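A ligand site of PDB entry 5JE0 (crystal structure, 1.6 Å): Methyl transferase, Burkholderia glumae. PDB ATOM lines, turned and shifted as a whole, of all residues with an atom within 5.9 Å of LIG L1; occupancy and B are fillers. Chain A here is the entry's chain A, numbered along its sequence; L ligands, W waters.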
ATOM      1  N   TYR A   9       6.036  22.552  -5.016  1.00  0.00           N
ATOM      2  CA  TYR A   9       7.399  23.021  -5.162  1.00  0.00           C
ATOM      3  C   TYR A   9       7.970  23.585  -3.876  1.00  0.00           C
ATOM      4  O   TYR A   9       9.167  23.905  -3.837  1.00  0.00           O
ATOM      5  CB  TYR A   9       7.491  24.059  -6.298  1.00  0.00           C
ATOM      6  CG  TYR A   9       7.645  23.416  -7.659  1.00  0.00           C
ATOM      7  CD1 TYR A   9       8.855  23.483  -8.359  1.00  0.00           C
ATOM      8  CD2 TYR A   9       6.593  22.718  -8.237  1.00  0.00           C
ATOM      9  CE1 TYR A   9       8.991  22.879  -9.623  1.00  0.00           C
ATOM     10  CE2 TYR A   9       6.713  22.112  -9.485  1.00  0.00           C
ATOM     11  CZ  TYR A   9       7.912  22.198 -10.168  1.00  0.00           C
ATOM     12  OH  TYR A   9       8.038  21.594 -11.404  1.00  0.00           O
ATOM     13  N   PHE A  16      15.200  22.953  -7.989  1.00  0.00           N
ATOM     14  CA  PHE A  16      14.719  23.158  -9.351  1.00  0.00           C
ATOM     15  C   PHE A  16      15.763  23.881 -10.192  1.00  0.00           C
ATOM     16  O   PHE A  16      15.962  23.541 -11.364  1.00  0.00           O
ATOM     17  CB  PHE A  16      13.382  23.911  -9.358  1.00  0.00           C
ATOM     18  CG  PHE A  16      12.911  24.265 -10.731  1.00  0.00           C
ATOM     19  CD1 PHE A  16      12.371  23.280 -11.567  1.00  0.00           C
ATOM     20  CD2 PHE A  16      13.037  25.554 -11.220  1.00  0.00           C
ATOM     21  CE1 PHE A  16      11.955  23.594 -12.847  1.00  0.00           C
ATOM     22  CE2 PHE A  16      12.621  25.868 -12.500  1.00  0.00           C
ATOM     23  CZ  PHE A  16      12.078  24.887 -13.320  1.00  0.00           C
ATOM     24  N   PHE A  19      18.224  21.458 -11.306  1.00  0.00           N
ATOM     25  CA  PHE A  19      17.760  20.736 -12.483  1.00  0.00           C
ATOM     26  C   PHE A  19      17.958  21.555 -13.744  1.00  0.00           C
ATOM     27  O   PHE A  19      18.430  21.026 -14.767  1.00  0.00           O
ATOM     28  CB  PHE A  19      16.289  20.359 -12.290  1.00  0.00           C
ATOM     29  CG  PHE A  19      15.498  20.305 -13.552  1.00  0.00           C
ATOM     30  CD1 PHE A  19      15.607  19.213 -14.422  1.00  0.00           C
ATOM     31  CD2 PHE A  19      14.643  21.339 -13.886  1.00  0.00           C
ATOM     32  CE1 PHE A  19      14.880  19.162 -15.588  1.00  0.00           C
ATOM     33  CE2 PHE A  19      13.900  21.287 -15.060  1.00  0.00           C
ATOM     34  CZ  PHE A  19      14.025  20.195 -15.921  1.00  0.00           C
ATOM     35  N   THR A  20      17.640  22.862 -13.707  1.00  0.00           N
ATOM     36  CA  THR A  20      17.753  23.654 -14.923  1.00  0.00           C
ATOM     37  C   THR A  20      19.200  23.801 -15.360  1.00  0.00           C
ATOM     38  O   THR A  20      19.450  24.037 -16.544  1.00  0.00           O
ATOM     39  CB  THR A  20      17.107  25.037 -14.757  1.00  0.00           C
ATOM     40  OG1 THR A  20      17.882  25.856 -13.870  1.00  0.00           O
ATOM     41  CG2 THR A  20      15.647  24.906 -14.254  1.00  0.00           C
ATOM     42  N   GLN A  25      17.640  18.995 -21.684  1.00  0.00           N
ATOM     43  CA  GLN A  25      16.515  19.583 -22.390  1.00  0.00           C
ATOM     44  C   GLN A  25      16.427  21.089 -22.206  1.00  0.00           C
ATOM     45  O   GLN A  25      15.823  21.768 -23.044  1.00  0.00           O
ATOM     46  CB  GLN A  25      15.205  18.958 -21.929  1.00  0.00           C
ATOM     47  CG  GLN A  25      14.806  19.313 -20.508  1.00  0.00           C
ATOM     48  CD  GLN A  25      13.417  18.854 -20.170  1.00  0.00           C
ATOM     49  OE1 GLN A  25      13.027  17.752 -20.554  1.00  0.00           O
ATOM     50  NE2 GLN A  25      12.652  19.674 -19.458  1.00  0.00           N
ATOM     51  N   ARG A  26      17.005  21.620 -21.122  1.00  0.00           N
ATOM     52  CA  ARG A  26      16.745  23.001 -20.747  1.00  0.00           C
ATOM     53  C   ARG A  26      17.319  23.987 -21.764  1.00  0.00           C
ATOM     54  O   ARG A  26      16.692  24.996 -22.071  1.00  0.00           O
ATOM     55  CB  ARG A  26      17.300  23.277 -19.357  1.00  0.00           C
ATOM     56  CG  ARG A  26      17.000  24.702 -18.837  1.00  0.00           C
ATOM     57  CD  ARG A  26      15.496  24.954 -18.643  1.00  0.00           C
ATOM     58  NE  ARG A  26      15.312  26.188 -17.878  1.00  0.00           N
ATOM     59  CZ  ARG A  26      14.180  26.599 -17.317  1.00  0.00           C
ATOM     60  NH1 ARG A  26      13.056  25.888 -17.416  1.00  0.00           N
ATOM     61  NH2 ARG A  26      14.173  27.734 -16.638  1.00  0.00           N
ATOM     62  N   GLU A  29      14.822  24.145 -24.654  1.00  0.00           N
ATOM     63  CA  GLU A  29      13.579  24.850 -24.370  1.00  0.00           C
ATOM     64  C   GLU A  29      13.816  26.344 -24.192  1.00  0.00           C
ATOM     65  O   GLU A  29      12.999  27.155 -24.657  1.00  0.00           O
ATOM     66  CB  GLU A  29      12.881  24.226 -23.147  1.00  0.00           C
ATOM     67  CG  GLU A  29      13.300  24.674 -21.784  1.00  0.00           C
ATOM     68  CD  GLU A  29      12.684  23.819 -20.687  1.00  0.00           C
ATOM     69  OE1 GLU A  29      12.639  22.581 -20.855  1.00  0.00           O
ATOM     70  OE2 GLU A  29      12.241  24.383 -19.660  1.00  0.00           O
ATOM     71  N   ALA A 113       5.910  29.338 -19.098  1.00  0.00           N
ATOM     72  CA  ALA A 113       6.744  28.146 -19.262  1.00  0.00           C
ATOM     73  C   ALA A 113       6.404  27.173 -18.142  1.00  0.00           C
ATOM     74  O   ALA A 113       6.736  27.414 -16.975  1.00  0.00           O
ATOM     75  CB  ALA A 113       8.222  28.500 -19.272  1.00  0.00           C
ATOM     76  N   TRP A 114       5.730  26.077 -18.499  1.00  0.00           N
ATOM     77  CA  TRP A 114       5.337  25.013 -17.567  1.00  0.00           C
ATOM     78  C   TRP A 114       4.243  25.486 -16.609  1.00  0.00           C
ATOM     79  O   TRP A 114       4.309  25.239 -15.402  1.00  0.00           O
ATOM     80  CB  TRP A 114       6.542  24.465 -16.819  1.00  0.00           C
ATOM     81  CG  TRP A 114       7.612  24.006 -17.761  1.00  0.00           C
ATOM     82  CD1 TRP A 114       8.841  24.548 -17.915  1.00  0.00           C
ATOM     83  CD2 TRP A 114       7.513  22.937 -18.690  1.00  0.00           C
ATOM     84  NE1 TRP A 114       9.541  23.869 -18.887  1.00  0.00           N
ATOM     85  CE2 TRP A 114       8.747  22.865 -19.381  1.00  0.00           C
ATOM     86  CE3 TRP A 114       6.490  22.014 -19.006  1.00  0.00           C
ATOM     87  CZ2 TRP A 114       9.007  21.896 -20.361  1.00  0.00           C
ATOM     88  CZ3 TRP A 114       6.736  21.070 -19.977  1.00  0.00           C
ATOM     89  CH2 TRP A 114       7.983  21.017 -20.646  1.00  0.00           C
ATOM     90  N   ASN A 117       0.488  22.463 -17.872  1.00  0.00           N
ATOM     91  CA  ASN A 117       0.594  21.087 -17.400  1.00  0.00           C
ATOM     92  C   ASN A 117       0.358  20.937 -15.908  1.00  0.00           C
ATOM     93  O   ASN A 117       0.379  19.809 -15.399  1.00  0.00           O
ATOM     94  CB  ASN A 117       1.959  20.484 -17.801  1.00  0.00           C
ATOM     95  CG  ASN A 117       3.162  21.229 -17.223  1.00  0.00           C
ATOM     96  OD1 ASN A 117       3.207  22.453 -17.203  1.00  0.00           O
ATOM     97  ND2 ASN A 117       4.164  20.464 -16.782  1.00  0.00           N
ATOM     98  N   TYR A 118       0.071  22.021 -15.191  1.00  0.00           N
ATOM     99  CA  TYR A 118      -0.341  21.900 -13.813  1.00  0.00           C
ATOM    100  C   TYR A 118      -1.843  22.075 -13.636  1.00  0.00           C
ATOM    101  O   TYR A 118      -2.337  21.916 -12.513  1.00  0.00           O
ATOM    102  CB  TYR A 118       0.436  22.904 -12.947  1.00  0.00           C
ATOM    103  CG  TYR A 118       1.857  22.466 -12.845  1.00  0.00           C
ATOM    104  CD1 TYR A 118       2.227  21.478 -11.939  1.00  0.00           C
ATOM    105  CD2 TYR A 118       2.833  22.971 -13.705  1.00  0.00           C
ATOM    106  CE1 TYR A 118       3.536  21.015 -11.883  1.00  0.00           C
ATOM    107  CE2 TYR A 118       4.128  22.508 -13.657  1.00  0.00           C
ATOM    108  CZ  TYR A 118       4.473  21.521 -12.757  1.00  0.00           C
ATOM    109  OH  TYR A 118       5.779  21.050 -12.705  1.00  0.00           O
ATOM    110  N   VAL A 147       3.545  20.382 -21.879  1.00  0.00           N
ATOM    111  CA  VAL A 147       3.674  18.978 -22.268  1.00  0.00           C
ATOM    112  C   VAL A 147       3.058  18.754 -23.641  1.00  0.00           C
ATOM    113  O   VAL A 147       1.938  19.188 -23.914  1.00  0.00           O
ATOM    114  CB  VAL A 147       3.029  18.089 -21.199  1.00  0.00           C
ATOM    115  CG1 VAL A 147       2.931  16.630 -21.709  1.00  0.00           C
ATOM    116  CG2 VAL A 147       3.803  18.171 -19.886  1.00  0.00           C
ATOM    117  N   VAL A 163      14.278  14.784 -17.065  1.00  0.00           N
ATOM    118  CA  VAL A 163      12.969  14.577 -16.434  1.00  0.00           C
ATOM    119  C   VAL A 163      12.653  13.093 -16.467  1.00  0.00           C
ATOM    120  O   VAL A 163      12.333  12.540 -17.531  1.00  0.00           O
ATOM    121  CB  VAL A 163      11.853  15.390 -17.109  1.00  0.00           C
ATOM    122  CG1 VAL A 163      10.527  15.075 -16.449  1.00  0.00           C
ATOM    123  CG2 VAL A 163      12.152  16.881 -16.991  1.00  0.00           C
ATOM    124  N   PHE A 181      12.570  15.519 -11.315  1.00  0.00           N
ATOM    125  CA  PHE A 181      13.721  16.121 -11.959  1.00  0.00           C
ATOM    126  C   PHE A 181      14.971  15.344 -11.551  1.00  0.00           C
ATOM    127  O   PHE A 181      15.068  14.849 -10.429  1.00  0.00           O
ATOM    128  CB  PHE A 181      13.856  17.597 -11.548  1.00  0.00           C
ATOM    129  CG  PHE A 181      12.650  18.434 -11.902  1.00  0.00           C
ATOM    130  CD1 PHE A 181      12.372  18.750 -13.222  1.00  0.00           C
ATOM    131  CD2 PHE A 181      11.817  18.925 -10.909  1.00  0.00           C
ATOM    132  CE1 PHE A 181      11.301  19.540 -13.549  1.00  0.00           C
ATOM    133  CE2 PHE A 181      10.733  19.707 -11.237  1.00  0.00           C
ATOM    134  CZ  PHE A 181      10.466  20.017 -12.553  1.00  0.00           C
ATOM    135  N   PHE A 189       7.601  15.590  -8.667  1.00  0.00           N
ATOM    136  CA  PHE A 189       6.501  16.470  -9.022  1.00  0.00           C
ATOM    137  C   PHE A 189       5.522  15.685  -9.885  1.00  0.00           C
ATOM    138  O   PHE A 189       5.835  14.620 -10.419  1.00  0.00           O
ATOM    139  CB  PHE A 189       6.995  17.751  -9.704  1.00  0.00           C
ATOM    140  CG  PHE A 189       7.569  17.546 -11.085  1.00  0.00           C
ATOM    141  CD1 PHE A 189       6.873  17.993 -12.198  1.00  0.00           C
ATOM    142  CD2 PHE A 189       8.797  16.933 -11.261  1.00  0.00           C
ATOM    143  CE1 PHE A 189       7.371  17.827 -13.464  1.00  0.00           C
ATOM    144  CE2 PHE A 189       9.324  16.757 -12.531  1.00  0.00           C
ATOM    145  CZ  PHE A 189       8.610  17.207 -13.636  1.00  0.00           C
ATOM    146  N   PHE A 191       2.334  16.160 -12.947  1.00  0.00           N
ATOM    147  CA  PHE A 191       1.780  17.068 -13.941  1.00  0.00           C
ATOM    148  C   PHE A 191       0.756  16.304 -14.764  1.00  0.00           C
ATOM    149  O   PHE A 191       0.589  15.094 -14.635  1.00  0.00           O
ATOM    150  CB  PHE A 191       2.892  17.685 -14.840  1.00  0.00           C
ATOM    151  CG  PHE A 191       3.667  16.673 -15.653  1.00  0.00           C
ATOM    152  CD1 PHE A 191       3.228  16.248 -16.894  1.00  0.00           C
ATOM    153  CD2 PHE A 191       4.857  16.155 -15.158  1.00  0.00           C
ATOM    154  CE1 PHE A 191       3.950  15.329 -17.638  1.00  0.00           C
ATOM    155  CE2 PHE A 191       5.581  15.230 -15.895  1.00  0.00           C
ATOM    156  CZ  PHE A 191       5.134  14.820 -17.134  1.00  0.00           C
ATOM    157  N   LEU A 239       8.536  15.149 -24.894  1.00  0.00           N
ATOM    158  CA  LEU A 239       7.691  15.490 -23.763  1.00  0.00           C
ATOM    159  C   LEU A 239       7.210  16.936 -23.805  1.00  0.00           C
ATOM    160  O   LEU A 239       6.214  17.258 -23.148  1.00  0.00           O
ATOM    161  CB  LEU A 239       8.458  15.236 -22.460  1.00  0.00           C
ATOM    162  CG  LEU A 239       7.781  15.520 -21.119  1.00  0.00           C
ATOM    163  CD1 LEU A 239       6.425  14.757 -21.044  1.00  0.00           C
ATOM    164  CD2 LEU A 239       8.692  15.064 -20.040  1.00  0.00           C
ATOM    165  N   GLN A 240       7.867  17.793 -24.573  1.00  0.00           N
ATOM    166  CA  GLN A 240       7.625  19.222 -24.485  1.00  0.00           C
ATOM    167  C   GLN A 240       7.252  19.816 -25.832  1.00  0.00           C
ATOM    168  O   GLN A 240       7.586  19.281 -26.893  1.00  0.00           O
ATOM    169  CB  GLN A 240       8.863  19.933 -23.916  1.00  0.00           C
ATOM    170  CG  GLN A 240      10.140  19.732 -24.712  1.00  0.00           C
ATOM    171  CD  GLN A 240      11.306  20.448 -24.080  1.00  0.00           C
ATOM    172  OE1 GLN A 240      11.956  21.256 -24.716  1.00  0.00           O
ATOM    173  NE2 GLN A 240      11.555  20.177 -22.795  1.00  0.00           N
HETATM  174  C1  LIG L   1       9.339  20.117 -17.341  1.00  0.00           C
HETATM  175  N1  LIG L   1       9.659  19.174 -18.219  1.00  0.00           N
HETATM  176  N2  LIG L   1       8.796  18.242 -18.465  1.00  0.00           N
HETATM  177  C2  LIG L   1       7.617  18.190 -17.878  1.00  0.00           C
HETATM  178  N3  LIG L   1       7.228  19.082 -16.989  1.00  0.00           N
HETATM  179  C3  LIG L   1       8.084  20.068 -16.703  1.00  0.00           C
HETATM  180  C4  LIG L   1       7.772  21.121 -15.723  1.00  0.00           C
HETATM  181  O1  LIG L   1       6.697  21.176 -15.142  1.00  0.00           O
HETATM  182  N4  LIG L   1       8.704  22.090 -15.485  1.00  0.00           N
HETATM  183  C5  LIG L   1       9.890  22.090 -16.136  1.00  0.00           C
HETATM  184  O2  LIG L   1      10.713  22.964 -15.907  1.00  0.00           O
HETATM  185  N5  LIG L   1      10.225  21.150 -17.030  1.00  0.00           N
HETATM  186  N1  LG2 L   2       8.596  28.877 -15.205  1.00  0.00           N
HETATM  187  C1  LG2 L   2       9.730  28.404 -14.344  1.00  0.00           C
HETATM  188  C2  LG2 L   2       9.349  27.255 -13.401  1.00  0.00           C
HETATM  189  C3  LG2 L   2       8.679  26.058 -14.095  1.00  0.00           C
HETATM  190  S1  LG2 L   2       8.398  24.725 -12.971  1.00  0.00           S
HETATM  191  C4  LG2 L   2      10.891  27.988 -15.194  1.00  0.00           C
HETATM  192  O1  LG2 L   2      12.069  28.226 -14.829  1.00  0.00           O
HETATM  193  O2  LG2 L   2      10.663  27.412 -16.265  1.00  0.00           O
HETATM  194  C5  LG2 L   2       6.644  24.844 -12.769  1.00  0.00           C
HETATM  195  C6  LG2 L   2       6.237  25.959 -11.806  1.00  0.00           C
HETATM  196  O3  LG2 L   2       4.812  26.128 -11.909  1.00  0.00           O
HETATM  197  C7  LG2 L   2       6.564  25.681 -10.334  1.00  0.00           C
HETATM  198  O4  LG2 L   2       7.339  26.789  -9.773  1.00  0.00           O
HETATM  199  C8  LG2 L   2       5.185  25.593  -9.687  1.00  0.00           C
HETATM  200  O5  LG2 L   2       5.116  26.026  -8.324  1.00  0.00           O
HETATM  201  C9  LG2 L   2       4.361  26.473 -10.606  1.00  0.00           C
HETATM  202  N2  LG2 L   2       2.915  26.182 -10.599  1.00  0.00           N
HETATM  203  C10 LG2 L   2       2.321  24.961 -10.588  1.00  0.00           C
HETATM  204  N3  LG2 L   2       0.977  25.103 -10.596  1.00  0.00           N
HETATM  205  C11 LG2 L   2       0.693  26.398 -10.628  1.00  0.00           C
HETATM  206  C12 LG2 L   2      -0.524  27.215 -10.664  1.00  0.00           C
HETATM  207  N4  LG2 L   2      -1.758  26.624 -10.656  1.00  0.00           N
HETATM  208  N5  LG2 L   2      -0.384  28.569 -10.682  1.00  0.00           N
HETATM  209  C13 LG2 L   2       0.841  29.162 -10.686  1.00  0.00           C
HETATM  210  N6  LG2 L   2       1.985  28.482 -10.644  1.00  0.00           N
HETATM  211  C14 LG2 L   2       1.972  27.117 -10.634  1.00  0.00           C
HETATM  212  O   HOH W   1      12.650  22.340 -17.898  1.00  0.00           O
HETATM  213  O   HOH W   2      10.365  17.977 -20.999  1.00  0.00           O
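The side-chain hydroxyl (OH) of Tyr 118 is in hydrogen-bond range of an oxygen (O1) of LIG L1 (2.6 Å).
O1 of LIG L1 is in hydrogen-bond range of ND2 of Asn 117 (3.1 Å).
NE1 of Trp 114 lies close to O2 of LIG L1, at 3.3 Å.
The side-chain amide nitrogen (NE2) of Gln 25 lies within hydrogen-bond range of a nitrogen (N1) of LIG L1 (3.3 Å).
The side-chain hydroxyl (OH) of Tyr 9 lies close to a sulfur (S1) of LG2 L2 (3.5 Å).
O1 of LG2 L2 is in salt-bridge range of NH2 of Arg 26, 2.8 Å away.
The backbone carbonyl oxygen (O) of Ala 113 is in hydrogen-bond range of a nitrogen (N1) of LG2 L2 (3.0 Å).
A nitrogen (N4) of LIG L1 sits close to a sulfur (S1) of LG2 L2 (3.7 Å).
The side-chain hydroxyl of Tyr 118 sits at hydrogen-bond distance from the side-chain hydroxyl of Tyr 9 (2.7 Å).
The side-chain amide oxygen of Asn 117 lies close to the backbone carbonyl oxygen of Trp 114 (3.5 Å).
The indole nitrogen (NE1) of Trp 114 is in hydrogen-bond range of the side-chain carboxylate (OE2) of Glu 29, 2.9 Å away.
OE1 of Glu 29 is in hydrogen-bond range of NE2 of Gln 25 (3.2 Å).
Residues that only touch LIG L1: Phe 16 (3.4 Å), Leu 239 (3.5 Å), Val 163 (3.6 Å), Phe 19 (3.7 Å), Phe 189 (3.7 Å), Phe 181 (3.9 Å) and Tyr 9 (3.99 Å).
Water W1 lies within hydrogen-bond range of OE2 of Glu 29 (2.7 Å), N5 of LIG L1 (2.8 Å) and NE2 of Gln 25 (3.1 Å).
Water W2 lies within hydrogen-bond range of the side-chain amide oxygen (OE1) of Gln 25, a nitrogen (N2) of LIG L1 and the side-chain amide nitrogen (NE2) of Gln 240.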
